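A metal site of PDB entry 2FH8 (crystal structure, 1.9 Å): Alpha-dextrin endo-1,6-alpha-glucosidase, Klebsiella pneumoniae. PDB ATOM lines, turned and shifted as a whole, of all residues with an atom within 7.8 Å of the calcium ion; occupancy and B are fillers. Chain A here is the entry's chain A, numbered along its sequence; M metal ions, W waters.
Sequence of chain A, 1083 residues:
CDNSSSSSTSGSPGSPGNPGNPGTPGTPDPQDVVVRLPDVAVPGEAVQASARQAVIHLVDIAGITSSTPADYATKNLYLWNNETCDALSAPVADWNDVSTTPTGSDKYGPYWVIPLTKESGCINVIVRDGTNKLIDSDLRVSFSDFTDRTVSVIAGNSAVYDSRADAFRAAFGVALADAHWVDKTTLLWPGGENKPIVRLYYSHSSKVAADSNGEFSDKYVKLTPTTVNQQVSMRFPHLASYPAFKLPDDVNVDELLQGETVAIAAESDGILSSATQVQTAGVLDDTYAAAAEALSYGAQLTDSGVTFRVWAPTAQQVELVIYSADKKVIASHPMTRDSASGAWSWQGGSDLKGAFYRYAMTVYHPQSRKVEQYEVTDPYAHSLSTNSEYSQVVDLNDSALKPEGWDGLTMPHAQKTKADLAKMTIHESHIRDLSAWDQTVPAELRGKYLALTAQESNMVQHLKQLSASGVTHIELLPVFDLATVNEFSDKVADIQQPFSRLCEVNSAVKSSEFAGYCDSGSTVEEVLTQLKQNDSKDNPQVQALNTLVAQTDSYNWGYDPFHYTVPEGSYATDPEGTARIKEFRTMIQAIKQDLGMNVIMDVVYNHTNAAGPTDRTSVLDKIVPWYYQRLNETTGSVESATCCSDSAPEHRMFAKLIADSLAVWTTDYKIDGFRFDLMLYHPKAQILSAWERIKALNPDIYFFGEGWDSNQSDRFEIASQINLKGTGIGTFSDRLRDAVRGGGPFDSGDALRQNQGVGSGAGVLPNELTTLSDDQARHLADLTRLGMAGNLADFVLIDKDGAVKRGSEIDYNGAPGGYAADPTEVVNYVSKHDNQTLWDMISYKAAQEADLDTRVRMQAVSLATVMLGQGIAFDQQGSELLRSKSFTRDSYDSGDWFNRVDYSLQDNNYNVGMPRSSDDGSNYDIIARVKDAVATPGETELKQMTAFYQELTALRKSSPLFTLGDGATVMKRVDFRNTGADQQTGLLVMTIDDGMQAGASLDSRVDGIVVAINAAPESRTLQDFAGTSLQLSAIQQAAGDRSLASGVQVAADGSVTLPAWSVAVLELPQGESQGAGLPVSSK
OD2 of Asp 1003 is in salt-bridge range of NH1 of Arg 1005 (3.7 Å). The backbone NH (N) of Asp 994 sits at hydrogen-bond distance from the backbone carbonyl oxygen (O) of Asp 1007 (3.0 Å). The side-chain carboxylate (OD1) of Asp 994 sits at hydrogen-bond distance from the backbone NH (N) of Leu 1002, 2.9 Å away. The backbone carbonyl oxygen of Asp 994 lies close to the side-chain amide oxygen of Gln 1074 (2.9 Å). NH1 of Arg 973 lies within salt-bridge range of OD1 of Asp 994, 2.9 Å away. N of Gln 1070 sits at hydrogen-bond distance from O of Arg 1005.
The nearest printed residue that does not touch the calcium ion is Ser 1004 (4.1 Å).
The calcium ion is bound by the backbone carbonyl oxygen (O) of Asp 1003 (2.1 Å), the side-chain carboxylate (OD2) of Asp 994 (2.2 Å), the side-chain amide oxygen (OE1) of Gln 1070 (2.2 Å), water W1 (2.3 Å), the backbone carbonyl oxygen (O) of Val 1006 (2.3 Å) and the side-chain hydroxyl (OG) of Ser 1001 (2.4 Å).
Water W1 lies within hydrogen-bond range of OD1 of Asp 1007 (2.6 Å) and O of Asp 994 (2.7 Å).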
ATOM      1  N   LEU A 961     -13.279  10.359   5.176  1.00  0.00           N
ATOM      2  CA  LEU A 961     -13.149  10.513   3.726  1.00  0.00           C
ATOM      3  C   LEU A 961     -12.869  11.971   3.322  1.00  0.00           C
ATOM      4  O   LEU A 961     -12.288  12.225   2.261  1.00  0.00           O
ATOM      5  CB  LEU A 961     -14.406   9.997   3.035  1.00  0.00           C
ATOM      6  CG  LEU A 961     -14.670   8.497   3.236  1.00  0.00           C
ATOM      7  CD1 LEU A 961     -16.012   8.111   2.629  1.00  0.00           C
ATOM      8  CD2 LEU A 961     -13.535   7.698   2.610  1.00  0.00           C
ATOM      9  N   ARG A 973      -9.136   8.203  -4.600  1.00  0.00           N
ATOM     10  CA  ARG A 973     -10.537   8.304  -4.199  1.00  0.00           C
ATOM     11  C   ARG A 973     -11.343   9.527  -4.616  1.00  0.00           C
ATOM     12  O   ARG A 973     -12.561   9.447  -4.776  1.00  0.00           O
ATOM     13  CB  ARG A 973     -10.624   8.175  -2.671  1.00  0.00           C
ATOM     14  CG  ARG A 973     -10.078   6.859  -2.127  1.00  0.00           C
ATOM     15  CD  ARG A 973      -9.871   6.928  -0.628  1.00  0.00           C
ATOM     16  NE  ARG A 973      -9.358   5.675  -0.078  1.00  0.00           N
ATOM     17  CZ  ARG A 973     -10.100   4.719   0.475  1.00  0.00           C
ATOM     18  NH1 ARG A 973     -11.419   4.867   0.556  1.00  0.00           N
ATOM     19  NH2 ARG A 973      -9.530   3.622   0.948  1.00  0.00           N
ATOM     20  N   ASP A 993     -14.520   8.263  -3.088  1.00  0.00           N
ATOM     21  CA  ASP A 993     -14.756   6.820  -3.096  1.00  0.00           C
ATOM     22  C   ASP A 993     -14.316   6.064  -1.856  1.00  0.00           C
ATOM     23  O   ASP A 993     -13.298   6.370  -1.231  1.00  0.00           O
ATOM     24  CB  ASP A 993     -14.073   6.198  -4.321  1.00  0.00           C
ATOM     25  CG  ASP A 993     -14.475   4.750  -4.556  1.00  0.00           C
ATOM     26  OD1 ASP A 993     -13.749   4.045  -5.277  1.00  0.00           O
ATOM     27  OD2 ASP A 993     -15.521   4.311  -4.024  1.00  0.00           O
ATOM     28  N   ASP A 994     -15.092   5.050  -1.497  1.00  0.00           N
ATOM     29  CA  ASP A 994     -14.772   4.184  -0.365  1.00  0.00           C
ATOM     30  C   ASP A 994     -15.230   2.784  -0.750  1.00  0.00           C
ATOM     31  O   ASP A 994     -15.356   1.902   0.097  1.00  0.00           O
ATOM     32  CB  ASP A 994     -15.478   4.654   0.907  1.00  0.00           C
ATOM     33  CG  ASP A 994     -14.862   4.062   2.164  1.00  0.00           C
ATOM     34  OD1 ASP A 994     -13.633   4.162   2.332  1.00  0.00           O
ATOM     35  OD2 ASP A 994     -15.614   3.480   2.984  1.00  0.00           O
ATOM     36  N   GLY A 995     -15.462   2.609  -2.042  1.00  0.00           N
ATOM     37  CA  GLY A 995     -15.904   1.326  -2.562  1.00  0.00           C
ATOM     38  C   GLY A 995     -14.750   0.352  -2.740  1.00  0.00           C
ATOM     39  O   GLY A 995     -13.595   0.693  -2.503  1.00  0.00           O
ATOM     40  N   ALA A1000      -9.251  -0.164   1.032  1.00  0.00           N
ATOM     41  CA  ALA A1000      -9.854  -0.459   2.319  1.00  0.00           C
ATOM     42  C   ALA A1000     -10.992   0.483   2.672  1.00  0.00           C
ATOM     43  O   ALA A1000     -10.941   1.671   2.367  1.00  0.00           O
ATOM     44  CB  ALA A1000      -8.784  -0.404   3.406  1.00  0.00           C
ATOM     45  N   SER A1001     -12.015  -0.053   3.323  1.00  0.00           N
ATOM     46  CA  SER A1001     -13.156   0.766   3.732  1.00  0.00           C
ATOM     47  C   SER A1001     -12.734   1.602   4.925  1.00  0.00           C
ATOM     48  O   SER A1001     -12.413   1.065   5.987  1.00  0.00           O
ATOM     49  CB  SER A1001     -14.343  -0.130   4.125  1.00  0.00           C
ATOM     50  OG  SER A1001     -15.386   0.634   4.696  1.00  0.00           O
ATOM     51  N   LEU A1002     -12.725   2.922   4.751  1.00  0.00           N
ATOM     52  CA  LEU A1002     -12.329   3.814   5.836  1.00  0.00           C
ATOM     53  C   LEU A1002     -13.516   4.256   6.675  1.00  0.00           C
ATOM     54  O   LEU A1002     -13.357   4.684   7.817  1.00  0.00           O
ATOM     55  CB  LEU A1002     -11.620   5.041   5.260  1.00  0.00           C
ATOM     56  CG  LEU A1002     -10.400   4.773   4.367  1.00  0.00           C
ATOM     57  CD1 LEU A1002      -9.808   6.089   3.882  1.00  0.00           C
ATOM     58  CD2 LEU A1002      -9.371   3.983   5.137  1.00  0.00           C
ATOM     59  N   ASP A1003     -14.715   4.145   6.108  1.00  0.00           N
ATOM     60  CA  ASP A1003     -15.935   4.549   6.811  1.00  0.00           C
ATOM     61  C   ASP A1003     -16.941   3.395   6.774  1.00  0.00           C
ATOM     62  O   ASP A1003     -17.495   3.078   5.729  1.00  0.00           O
ATOM     63  CB  ASP A1003     -16.517   5.799   6.137  1.00  0.00           C
ATOM     64  CG  ASP A1003     -17.589   6.461   6.971  1.00  0.00           C
ATOM     65  OD1 ASP A1003     -17.830   7.676   6.753  1.00  0.00           O
ATOM     66  OD2 ASP A1003     -18.201   5.793   7.835  1.00  0.00           O
ATOM     67  N   SER A1004     -17.178   2.775   7.936  1.00  0.00           N
ATOM     68  CA  SER A1004     -18.093   1.642   8.009  1.00  0.00           C
ATOM     69  C   SER A1004     -19.555   1.972   7.726  1.00  0.00           C
ATOM     70  O   SER A1004     -20.363   1.069   7.526  1.00  0.00           O
ATOM     71  CB  SER A1004     -17.994   0.985   9.393  1.00  0.00           C
ATOM     72  OG  SER A1004     -18.416   1.860  10.431  1.00  0.00           O
ATOM     73  N   ARG A1005     -19.886   3.253   7.673  1.00  0.00           N
ATOM     74  CA  ARG A1005     -21.274   3.662   7.427  1.00  0.00           C
ATOM     75  C   ARG A1005     -21.622   3.951   5.973  1.00  0.00           C
ATOM     76  O   ARG A1005     -22.786   3.873   5.598  1.00  0.00           O
ATOM     77  CB  ARG A1005     -21.597   4.893   8.271  1.00  0.00           C
ATOM     78  CG  ARG A1005     -21.185   4.784   9.727  1.00  0.00           C
ATOM     79  CD  ARG A1005     -20.297   5.949  10.111  1.00  0.00           C
ATOM     80  NE  ARG A1005     -21.017   7.219  10.019  1.00  0.00           N
ATOM     81  CZ  ARG A1005     -20.419   8.410  10.035  1.00  0.00           C
ATOM     82  NH1 ARG A1005     -19.099   8.487  10.140  1.00  0.00           N
ATOM     83  NH2 ARG A1005     -21.146   9.520   9.954  1.00  0.00           N
ATOM     84  N   VAL A1006     -20.623   4.280   5.160  1.00  0.00           N
ATOM     85  CA  VAL A1006     -20.866   4.606   3.768  1.00  0.00           C
ATOM     86  C   VAL A1006     -19.845   4.022   2.792  1.00  0.00           C
ATOM     87  O   VAL A1006     -18.736   3.669   3.183  1.00  0.00           O
ATOM     88  CB  VAL A1006     -20.894   6.144   3.561  1.00  0.00           C
ATOM     89  CG1 VAL A1006     -21.789   6.797   4.592  1.00  0.00           C
ATOM     90  CG2 VAL A1006     -19.480   6.706   3.659  1.00  0.00           C
ATOM     91  N   ASP A1007     -20.238   3.946   1.521  1.00  0.00           N
ATOM     92  CA  ASP A1007     -19.388   3.440   0.460  1.00  0.00           C
ATOM     93  C   ASP A1007     -18.855   4.594  -0.382  1.00  0.00           C
ATOM     94  O   ASP A1007     -18.038   4.403  -1.278  1.00  0.00           O
ATOM     95  CB  ASP A1007     -20.161   2.488  -0.462  1.00  0.00           C
ATOM     96  CG  ASP A1007     -20.473   1.170   0.202  1.00  0.00           C
ATOM     97  OD1 ASP A1007     -19.549   0.571   0.798  1.00  0.00           O
ATOM     98  OD2 ASP A1007     -21.638   0.727   0.114  1.00  0.00           O
ATOM     99  N   GLY A1008     -19.351   5.797  -0.099  1.00  0.00           N
ATOM    100  CA  GLY A1008     -18.913   6.956  -0.850  1.00  0.00           C
ATOM    101  C   GLY A1008     -19.673   8.194  -0.453  1.00  0.00           C
ATOM    102  O   GLY A1008     -20.766   8.111   0.119  1.00  0.00           O
ATOM    103  N   LEU A1068     -23.663   7.165   0.251  1.00  0.00           N
ATOM    104  CA  LEU A1068     -24.117   5.852  -0.185  1.00  0.00           C
ATOM    105  C   LEU A1068     -24.046   4.969   1.050  1.00  0.00           C
ATOM    106  O   LEU A1068     -22.962   4.568   1.475  1.00  0.00           O
ATOM    107  CB  LEU A1068     -23.199   5.272  -1.262  1.00  0.00           C
ATOM    108  CG  LEU A1068     -23.142   5.938  -2.638  1.00  0.00           C
ATOM    109  CD1 LEU A1068     -22.120   5.215  -3.510  1.00  0.00           C
ATOM    110  CD2 LEU A1068     -24.510   5.881  -3.293  1.00  0.00           C
ATOM    111  N   PRO A1069     -25.211   4.670   1.661  1.00  0.00           N
ATOM    112  CA  PRO A1069     -25.185   3.821   2.858  1.00  0.00           C
ATOM    113  C   PRO A1069     -24.525   2.480   2.558  1.00  0.00           C
ATOM    114  O   PRO A1069     -24.850   1.828   1.564  1.00  0.00           O
ATOM    115  CB  PRO A1069     -26.667   3.683   3.204  1.00  0.00           C
ATOM    116  CG  PRO A1069     -27.339   3.778   1.859  1.00  0.00           C
ATOM    117  CD  PRO A1069     -26.583   4.922   1.219  1.00  0.00           C
ATOM    118  N   GLN A1070     -23.573   2.083   3.400  1.00  0.00           N
ATOM    119  CA  GLN A1070     -22.861   0.824   3.210  1.00  0.00           C
ATOM    120  C   GLN A1070     -23.711  -0.360   3.653  1.00  0.00           C
ATOM    121  O   GLN A1070     -24.306  -0.346   4.733  1.00  0.00           O
ATOM    122  CB  GLN A1070     -21.548   0.836   3.992  1.00  0.00           C
ATOM    123  CG  GLN A1070     -20.647  -0.353   3.704  1.00  0.00           C
ATOM    124  CD  GLN A1070     -19.369  -0.319   4.504  1.00  0.00           C
ATOM    125  OE1 GLN A1070     -18.651   0.688   4.495  1.00  0.00           O
ATOM    126  NE2 GLN A1070     -19.061  -1.405   5.203  1.00  0.00           N
ATOM    127  N   GLY A1071     -23.752  -1.394   2.818  1.00  0.00           N
ATOM    128  CA  GLY A1071     -24.544  -2.570   3.138  1.00  0.00           C
ATOM    129  C   GLY A1071     -23.822  -3.577   4.015  1.00  0.00           C
ATOM    130  O   GLY A1071     -23.001  -3.207   4.866  1.00  0.00           O
ATOM    131  N   SER A1073     -21.637  -5.538   3.116  1.00  0.00           N
ATOM    132  CA  SER A1073     -20.231  -5.509   2.738  1.00  0.00           C
ATOM    133  C   SER A1073     -19.934  -4.262   1.915  1.00  0.00           C
ATOM    134  O   SER A1073     -20.833  -3.526   1.533  1.00  0.00           O
ATOM    135  CB  SER A1073     -19.887  -6.765   1.934  1.00  0.00           C
ATOM    136  OG  SER A1073     -18.529  -6.757   1.522  1.00  0.00           O
ATOM    137  N   GLN A1074     -18.650  -4.035   1.655  1.00  0.00           N
ATOM    138  CA  GLN A1074     -18.213  -2.886   0.868  1.00  0.00           C
ATOM    139  C   GLN A1074     -18.891  -2.909  -0.492  1.00  0.00           C
ATOM    140  O   GLN A1074     -18.914  -3.944  -1.171  1.00  0.00           O
ATOM    141  CB  GLN A1074     -16.689  -2.939   0.706  1.00  0.00           C
ATOM    142  CG  GLN A1074     -16.062  -1.655   0.181  1.00  0.00           C
ATOM    143  CD  GLN A1074     -14.548  -1.686   0.226  1.00  0.00           C
ATOM    144  OE1 GLN A1074     -13.895  -0.653   0.088  1.00  0.00           O
ATOM    145  NE2 GLN A1074     -13.979  -2.869   0.410  1.00  0.00           N
ATOM    146  N   GLY A1075     -19.454  -1.776  -0.891  1.00  0.00           N
ATOM    147  CA  GLY A1075     -20.146  -1.703  -2.166  1.00  0.00           C
ATOM    148  C   GLY A1075     -19.307  -1.159  -3.305  1.00  0.00           C
ATOM    149  O   GLY A1075     -18.089  -1.000  -3.175  1.00  0.00           O
HETATM  150 CA    CA M   1     -17.107   2.181   3.926  1.00  0.00          CA
HETATM  151  O   HOH W   1     -17.264   1.234   1.882  1.00  0.00           O
